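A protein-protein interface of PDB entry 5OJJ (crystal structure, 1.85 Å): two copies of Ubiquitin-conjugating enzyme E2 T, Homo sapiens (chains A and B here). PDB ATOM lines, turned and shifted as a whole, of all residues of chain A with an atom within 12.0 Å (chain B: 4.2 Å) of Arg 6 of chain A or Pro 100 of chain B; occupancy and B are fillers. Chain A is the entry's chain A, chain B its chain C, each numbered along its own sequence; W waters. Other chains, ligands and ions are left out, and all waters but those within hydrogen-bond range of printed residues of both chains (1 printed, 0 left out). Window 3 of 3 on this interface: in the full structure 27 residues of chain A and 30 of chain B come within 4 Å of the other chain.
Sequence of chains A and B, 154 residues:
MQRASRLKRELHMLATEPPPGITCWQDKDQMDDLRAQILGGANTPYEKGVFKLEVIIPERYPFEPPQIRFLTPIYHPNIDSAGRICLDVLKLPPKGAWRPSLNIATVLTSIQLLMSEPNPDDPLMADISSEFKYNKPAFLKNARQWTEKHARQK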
ATOM      1  N   ALA A   4      21.302  20.600 -12.762  1.00  0.00           N
ATOM      2  CA  ALA A   4      20.434  20.912 -13.945  1.00  0.00           C
ATOM      3  C   ALA A   4      20.975  22.111 -14.706  1.00  0.00           C
ATOM      4  O   ALA A   4      21.270  22.009 -15.900  1.00  0.00           O
ATOM      5  CB  ALA A   4      18.996  21.166 -13.508  1.00  0.00           C
ATOM      6  N   SER A   5      21.129  23.222 -13.977  1.00  0.00           N
ATOM      7  CA  SER A   5      21.642  24.511 -14.489  1.00  0.00           C
ATOM      8  C   SER A   5      22.994  24.439 -15.207  1.00  0.00           C
ATOM      9  O   SER A   5      23.319  25.330 -16.015  1.00  0.00           O
ATOM     10  CB  SER A   5      21.767  25.507 -13.331  1.00  0.00           C
ATOM     11  OG  SER A   5      22.649  25.014 -12.339  1.00  0.00           O
ATOM     12  N   ARG A   6      23.784  23.414 -14.864  1.00  0.00           N
ATOM     13  CA  ARG A   6      25.028  23.097 -15.557  1.00  0.00           C
ATOM     14  C   ARG A   6      24.865  23.098 -17.074  1.00  0.00           C
ATOM     15  O   ARG A   6      25.665  23.715 -17.756  1.00  0.00           O
ATOM     16  CB  ARG A   6      25.614  21.750 -15.080  1.00  0.00           C
ATOM     17  CG  ARG A   6      26.606  21.108 -16.054  1.00  0.00           C
ATOM     18  CD  ARG A   6      27.654  20.216 -15.390  1.00  0.00           C
ATOM     19  NE  ARG A   6      28.328  19.363 -16.387  1.00  0.00           N
ATOM     20  CZ  ARG A   6      29.204  18.386 -16.123  1.00  0.00           C
ATOM     21  NH1 ARG A   6      29.570  18.104 -14.876  1.00  0.00           N
ATOM     22  NH2 ARG A   6      29.714  17.667 -17.131  1.00  0.00           N
ATOM     23  N   LEU A   7      23.844  22.419 -17.589  1.00  0.00           N
ATOM     24  CA  LEU A   7      23.725  22.227 -19.038  1.00  0.00           C
ATOM     25  C   LEU A   7      23.614  23.559 -19.780  1.00  0.00           C
ATOM     26  O   LEU A   7      24.269  23.753 -20.789  1.00  0.00           O
ATOM     27  CB  LEU A   7      22.551  21.298 -19.391  1.00  0.00           C
ATOM     28  CG  LEU A   7      22.401  20.892 -20.864  1.00  0.00           C
ATOM     29  CD1 LEU A   7      23.544  20.010 -21.345  1.00  0.00           C
ATOM     30  CD2 LEU A   7      21.063  20.182 -21.080  1.00  0.00           C
ATOM     31  N   LYS A   8      22.817  24.490 -19.260  1.00  0.00           N
ATOM     32  CA  LYS A   8      22.700  25.819 -19.888  1.00  0.00           C
ATOM     33  C   LYS A   8      24.032  26.577 -19.940  1.00  0.00           C
ATOM     34  O   LYS A   8      24.383  27.157 -20.971  1.00  0.00           O
ATOM     35  CB  LYS A   8      21.628  26.664 -19.191  1.00  0.00           C
ATOM     36  CG  LYS A   8      20.215  26.330 -19.649  1.00  0.00           C
ATOM     37  CD  LYS A   8      19.220  27.434 -19.319  1.00  0.00           C
ATOM     38  CE  LYS A   8      17.913  27.227 -20.068  1.00  0.00           C
ATOM     39  NZ  LYS A   8      16.932  28.305 -19.768  1.00  0.00           N
ATOM     40  N   ARG A   9      24.764  26.549 -18.830  1.00  0.00           N
ATOM     41  CA  ARG A   9      26.108  27.133 -18.743  1.00  0.00           C
ATOM     42  C   ARG A   9      27.104  26.435 -19.650  1.00  0.00           C
ATOM     43  O   ARG A   9      27.921  27.074 -20.318  1.00  0.00           O
ATOM     44  CB  ARG A   9      26.636  27.011 -17.316  1.00  0.00           C
ATOM     45  CG  ARG A   9      25.927  27.879 -16.286  1.00  0.00           C
ATOM     46  CD  ARG A   9      26.047  27.284 -14.886  1.00  0.00           C
ATOM     47  NE  ARG A   9      27.391  26.742 -14.625  1.00  0.00           N
ATOM     48  CZ  ARG A   9      27.678  25.694 -13.846  1.00  0.00           C
ATOM     49  NH1 ARG A   9      26.729  25.012 -13.202  1.00  0.00           N
ATOM     50  NH2 ARG A   9      28.948  25.313 -13.710  1.00  0.00           N
ATOM     51  N   GLU A  10      27.042  25.109 -19.632  1.00  0.00           N
ATOM     52  CA  GLU A  10      27.894  24.282 -20.475  1.00  0.00           C
ATOM     53  C   GLU A  10      27.771  24.624 -21.945  1.00  0.00           C
ATOM     54  O   GLU A  10      28.767  24.742 -22.667  1.00  0.00           O
ATOM     55  CB  GLU A  10      27.543  22.813 -20.286  1.00  0.00           C
ATOM     56  CG  GLU A  10      28.749  21.955 -20.405  1.00  0.00           C
ATOM     57  CD  GLU A  10      28.443  20.484 -20.303  1.00  0.00           C
ATOM     58  OE1 GLU A  10      29.083  19.754 -21.054  1.00  0.00           O
ATOM     59  OE2 GLU A  10      27.565  20.080 -19.503  1.00  0.00           O
ATOM     60  N   LEU A  11      26.528  24.755 -22.390  1.00  0.00           N
ATOM     61  CA  LEU A  11      26.246  25.075 -23.774  1.00  0.00           C
ATOM     62  C   LEU A  11      26.665  26.488 -24.140  1.00  0.00           C
ATOM     63  O   LEU A  11      27.142  26.723 -25.252  1.00  0.00           O
ATOM     64  CB  LEU A  11      24.771  24.820 -24.071  1.00  0.00           C
ATOM     65  CG  LEU A  11      24.334  23.349 -23.977  1.00  0.00           C
ATOM     66  CD1 LEU A  11      22.858  23.216 -24.300  1.00  0.00           C
ATOM     67  CD2 LEU A  11      25.146  22.431 -24.879  1.00  0.00           C
ATOM     68  N   HIS A  12      26.538  27.424 -23.195  1.00  0.00           N
ATOM     69  CA  HIS A  12      27.033  28.779 -23.422  1.00  0.00           C
ATOM     70  C   HIS A  12      28.517  28.749 -23.703  1.00  0.00           C
ATOM     71  O   HIS A  12      28.989  29.367 -24.664  1.00  0.00           O
ATOM     72  CB  HIS A  12      26.718  29.711 -22.244  1.00  0.00           C
ATOM     73  CG  HIS A  12      27.430  31.028 -22.306  1.00  0.00           C
ATOM     74  ND1 HIS A  12      27.202  31.949 -23.305  1.00  0.00           N
ATOM     75  CD2 HIS A  12      28.366  31.578 -21.497  1.00  0.00           C
ATOM     76  CE1 HIS A  12      27.974  33.006 -23.114  1.00  0.00           C
ATOM     77  NE2 HIS A  12      28.694  32.804 -22.025  1.00  0.00           N
ATOM     78  N   MET A  13      29.246  28.028 -22.867  1.00  0.00           N
ATOM     79  CA  MET A  13      30.690  27.903 -23.012  1.00  0.00           C
ATOM     80  C   MET A  13      31.091  27.193 -24.311  1.00  0.00           C
ATOM     81  O   MET A  13      32.003  27.656 -25.006  1.00  0.00           O
ATOM     82  CB  MET A  13      31.290  27.270 -21.750  1.00  0.00           C
ATOM     83  CG  MET A  13      31.175  28.238 -20.568  1.00  0.00           C
ATOM     84  SD  MET A  13      31.379  27.536 -18.921  1.00  0.00           S
ATOM     85  CE  MET A  13      33.109  27.082 -19.017  1.00  0.00           C
ATOM     86  N   LEU A  14      30.371  26.135 -24.687  1.00  0.00           N
ATOM     87  CA  LEU A  14      30.573  25.522 -26.013  1.00  0.00           C
ATOM     88  C   LEU A  14      30.292  26.463 -27.173  1.00  0.00           C
ATOM     89  O   LEU A  14      31.001  26.444 -28.174  1.00  0.00           O
ATOM     90  CB  LEU A  14      29.730  24.251 -26.204  1.00  0.00           C
ATOM     91  CG  LEU A  14      30.434  22.940 -25.886  1.00  0.00           C
ATOM     92  CD1 LEU A  14      29.420  21.814 -25.897  1.00  0.00           C
ATOM     93  CD2 LEU A  14      31.548  22.666 -26.877  1.00  0.00           C
ATOM     94  N   ALA A  15      29.265  27.290 -27.046  1.00  0.00           N
ATOM     95  CA  ALA A  15      28.917  28.238 -28.098  1.00  0.00           C
ATOM     96  C   ALA A  15      29.940  29.366 -28.300  1.00  0.00           C
ATOM     97  O   ALA A  15      30.179  29.777 -29.433  1.00  0.00           O
ATOM     98  CB  ALA A  15      27.539  28.813 -27.844  1.00  0.00           C
ATOM     99  N   THR A  16      30.552  29.857 -27.218  1.00  0.00           N
ATOM    100  CA  THR A  16      31.447  31.017 -27.301  1.00  0.00           C
ATOM    101  C   THR A  16      32.924  30.650 -27.447  1.00  0.00           C
ATOM    102  O   THR A  16      33.645  31.330 -28.163  1.00  0.00           O
ATOM    103  CB  THR A  16      31.298  31.941 -26.081  1.00  0.00           C
ATOM    104  OG1 THR A  16      31.436  31.175 -24.881  1.00  0.00           O
ATOM    105  CG2 THR A  16      29.943  32.636 -26.096  1.00  0.00           C
ATOM    106  N   CYS A  24      29.186  23.313 -31.631  1.00  0.00           N
ATOM    107  CA  CYS A  24      28.036  22.607 -31.024  1.00  0.00           C
ATOM    108  C   CYS A  24      26.913  23.610 -30.826  1.00  0.00           C
ATOM    109  O   CYS A  24      27.121  24.638 -30.170  1.00  0.00           O
ATOM    110  CB  CYS A  24      28.379  21.891 -29.692  1.00  0.00           C
ATOM    111  SG  CYS A  24      26.995  20.924 -28.922  1.00  0.00           S
ATOM    112  N   GLN A  26      22.206  24.299 -31.232  1.00  0.00           N
ATOM    113  CA  GLN A  26      20.841  23.741 -31.139  1.00  0.00           C
ATOM    114  C   GLN A  26      20.078  23.954 -32.470  1.00  0.00           C
ATOM    115  O   GLN A  26      19.976  25.085 -32.920  1.00  0.00           O
ATOM    116  CB  GLN A  26      20.110  24.435 -29.983  1.00  0.00           C
ATOM    117  CG  GLN A  26      19.353  23.520 -29.043  1.00  0.00           C
ATOM    118  CD  GLN A  26      18.904  24.199 -27.744  1.00  0.00           C
ATOM    119  OE1 GLN A  26      17.735  24.112 -27.383  1.00  0.00           O
ATOM    120  NE2 GLN A  26      19.831  24.851 -27.030  1.00  0.00           N
ATOM    121  N   TYR B  61      21.960  12.764 -17.217  1.00  0.00           N
ATOM    122  CA  TYR B  61      23.194  13.542 -17.412  1.00  0.00           C
ATOM    123  C   TYR B  61      23.324  14.481 -16.201  1.00  0.00           C
ATOM    124  O   TYR B  61      22.299  15.053 -15.803  1.00  0.00           O
ATOM    125  CB  TYR B  61      23.107  14.351 -18.703  1.00  0.00           C
ATOM    126  CG  TYR B  61      24.355  15.149 -19.012  1.00  0.00           C
ATOM    127  CD1 TYR B  61      25.467  14.542 -19.578  1.00  0.00           C
ATOM    128  CD2 TYR B  61      24.431  16.507 -18.705  1.00  0.00           C
ATOM    129  CE1 TYR B  61      26.617  15.256 -19.827  1.00  0.00           C
ATOM    130  CE2 TYR B  61      25.580  17.244 -18.969  1.00  0.00           C
ATOM    131  CZ  TYR B  61      26.663  16.620 -19.539  1.00  0.00           C
ATOM    132  OH  TYR B  61      27.810  17.334 -19.789  1.00  0.00           O
ATOM    133  N   PRO B  62      24.508  14.693 -15.606  1.00  0.00           N
ATOM    134  CA  PRO B  62      25.830  14.260 -16.073  1.00  0.00           C
ATOM    135  C   PRO B  62      26.320  12.942 -15.491  1.00  0.00           C
ATOM    136  O   PRO B  62      27.494  12.610 -15.663  1.00  0.00           O
ATOM    137  CB  PRO B  62      26.729  15.418 -15.615  1.00  0.00           C
ATOM    138  CG  PRO B  62      26.099  15.859 -14.329  1.00  0.00           C
ATOM    139  CD  PRO B  62      24.608  15.691 -14.526  1.00  0.00           C
ATOM    140  N   TRP B  98      33.238   7.273 -18.889  1.00  0.00           N
ATOM    141  CA  TRP B  98      32.410   8.460 -18.574  1.00  0.00           C
ATOM    142  C   TRP B  98      32.368   8.741 -17.052  1.00  0.00           C
ATOM    143  O   TRP B  98      32.191   7.816 -16.261  1.00  0.00           O
ATOM    144  CB  TRP B  98      30.941   8.338 -19.079  1.00  0.00           C
ATOM    145  CG  TRP B  98      30.147   9.528 -18.643  1.00  0.00           C
ATOM    146  CD1 TRP B  98      29.283   9.581 -17.578  1.00  0.00           C
ATOM    147  CD2 TRP B  98      30.239  10.870 -19.142  1.00  0.00           C
ATOM    148  NE1 TRP B  98      28.810  10.845 -17.414  1.00  0.00           N
ATOM    149  CE2 TRP B  98      29.395  11.666 -18.341  1.00  0.00           C
ATOM    150  CE3 TRP B  98      30.977  11.484 -20.174  1.00  0.00           C
ATOM    151  CZ2 TRP B  98      29.219  13.042 -18.561  1.00  0.00           C
ATOM    152  CZ3 TRP B  98      30.821  12.856 -20.378  1.00  0.00           C
ATOM    153  CH2 TRP B  98      29.938  13.619 -19.579  1.00  0.00           C
ATOM    154  N   ARG B  99      32.537  10.010 -16.687  1.00  0.00           N
ATOM    155  CA  ARG B  99      32.311  10.518 -15.326  1.00  0.00           C
ATOM    156  C   ARG B  99      31.700  11.923 -15.399  1.00  0.00           C
ATOM    157  O   ARG B  99      31.959  12.654 -16.361  1.00  0.00           O
ATOM    158  CB  ARG B  99      33.651  10.615 -14.574  1.00  0.00           C
ATOM    159  CG  ARG B  99      34.480   9.333 -14.507  1.00  0.00           C
ATOM    160  CD  ARG B  99      33.958   8.335 -13.487  1.00  0.00           C
ATOM    161  NE  ARG B  99      34.912   7.239 -13.327  1.00  0.00           N
ATOM    162  CZ  ARG B  99      35.068   6.218 -14.169  1.00  0.00           C
ATOM    163  NH1 ARG B  99      34.307   6.097 -15.270  1.00  0.00           N
ATOM    164  NH2 ARG B  99      35.990   5.306 -13.925  1.00  0.00           N
ATOM    165  N   PRO B 100      30.976  12.354 -14.341  1.00  0.00           N
ATOM    166  CA  PRO B 100      30.494  13.739 -14.308  1.00  0.00           C
ATOM    167  C   PRO B 100      31.581  14.819 -14.171  1.00  0.00           C
ATOM    168  O   PRO B 100      31.258  16.012 -14.289  1.00  0.00           O
ATOM    169  CB  PRO B 100      29.534  13.764 -13.117  1.00  0.00           C
ATOM    170  CG  PRO B 100      29.889  12.589 -12.278  1.00  0.00           C
ATOM    171  CD  PRO B 100      30.538  11.575 -13.165  1.00  0.00           C
ATOM    172  N   SER B 101      32.835  14.406 -13.954  1.00  0.00           N
ATOM    173  CA  SER B 101      34.016  15.292 -14.019  1.00  0.00           C
ATOM    174  C   SER B 101      34.591  15.473 -15.448  1.00  0.00           C
ATOM    175  O   SER B 101      35.617  16.155 -15.633  1.00  0.00           O
ATOM    176  CB  SER B 101      35.114  14.776 -13.073  1.00  0.00           C
ATOM    177  OG  SER B 101      35.520  13.464 -13.419  1.00  0.00           O
ATOM    178  N   LEU B 102      33.941  14.858 -16.446  1.00  0.00           N
ATOM    179  CA  LEU B 102      34.149  15.190 -17.862  1.00  0.00           C
ATOM    180  C   LEU B 102      32.903  15.924 -18.385  1.00  0.00           C
ATOM    181  O   LEU B 102      31.928  16.094 -17.645  1.00  0.00           O
ATOM    182  CB  LEU B 102      34.389  13.923 -18.681  1.00  0.00           C
ATOM    183  CG  LEU B 102      35.478  12.970 -18.201  1.00  0.00           C
ATOM    184  CD1 LEU B 102      35.333  11.658 -18.941  1.00  0.00           C
ATOM    185  CD2 LEU B 102      36.864  13.576 -18.403  1.00  0.00           C
ATOM    186  N   ASN B 103      32.938  16.364 -19.648  1.00  0.00           N
ATOM    187  CA  ASN B 103      31.835  17.161 -20.199  1.00  0.00           C
ATOM    188  C   ASN B 103      31.637  16.904 -21.694  1.00  0.00           C
ATOM    189  O   ASN B 103      32.379  16.108 -22.301  1.00  0.00           O
ATOM    190  CB  ASN B 103      32.046  18.673 -19.900  1.00  0.00           C
ATOM    191  CG  ASN B 103      33.248  19.249 -20.606  1.00  0.00           C
ATOM    192  OD1 ASN B 103      33.920  18.565 -21.375  1.00  0.00           O
ATOM    193  ND2 ASN B 103      33.545  20.519 -20.337  1.00  0.00           N
HETATM  194  O   HOH W   1      31.022  20.889 -22.682  1.00  0.00           O
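The side-chain carboxylate of Glu 10 of chain A lies within hydrogen-bond range of the side-chain hydroxyl of Tyr 61 of chain B. The guanidinium group of Arg 6 of chain A lies within hydrogen-bond range of the backbone carbonyl oxygen of Pro 100 of chain B, at 2.8 Å. NH2 of Arg 6 of chain A is in hydrogen-bond range of OH of Tyr 61 of chain B. The backbone carbonyl oxygen of Leu 102 of chain B sits at hydrogen-bond distance from the guanidinium group of Arg 6 of chain A.
NE1 of Trp 98 of chain B lies within hydrogen-bond range of O of Pro 62 of chain B. OE2 of Glu 10 of chain A lies within salt-bridge range of NE of Arg 6 of chain A (3.3 Å).
Among the printed residues, merely in contact across the chains: Glu 10 of chain A with Asn 103 of chain B (3.4 Å), Arg 6 of chain A with Asn 103 of chain B (3.8 Å) and Arg 6 of chain A with Pro 62 of chain B (3.9 Å).
Arg 6 of chain A touches just these residues of chain B: Tyr 61, Pro 62, Pro 100, Leu 102 and Asn 103. Pro 100 of chain B touches one residue of chain A. Of chain A, only Arg 6 comes within 4 Å of Pro 62 of chain B. No residue of chain A comes within 4 Å of Ser 101 of chain B. Of chain A, only Arg 6 (3.8 Å) and Glu 10 (3.4 Å) come within 4 Å of Asn 103 of chain B. Printed residues of chain A within 4 Å of Tyr 61 of chain B: Arg 6 (3.3 Å) and Glu 10 (2.8 Å). Of the printed residues of chain B, Glu 10 of chain A touches Tyr 61 and Asn 103. Ser 5 of chain A touches none of the printed residues of chain B. The nearest printed residue of chain B that does not touch Arg 6 of chain A is Trp 98 of chain B (4.7 Å).
No position is printed for both chains. Of the 7 pairs that touch across the chains among the printed residues, none has its exchanged pair printed and touching as well.
Water W1 lies within hydrogen-bond range of the side-chain carboxylate (OE1) of Glu 10 of chain A (2.8 Å) and the side-chain amide nitrogen (ND2) of Asn 103 of chain B (3.5 Å).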
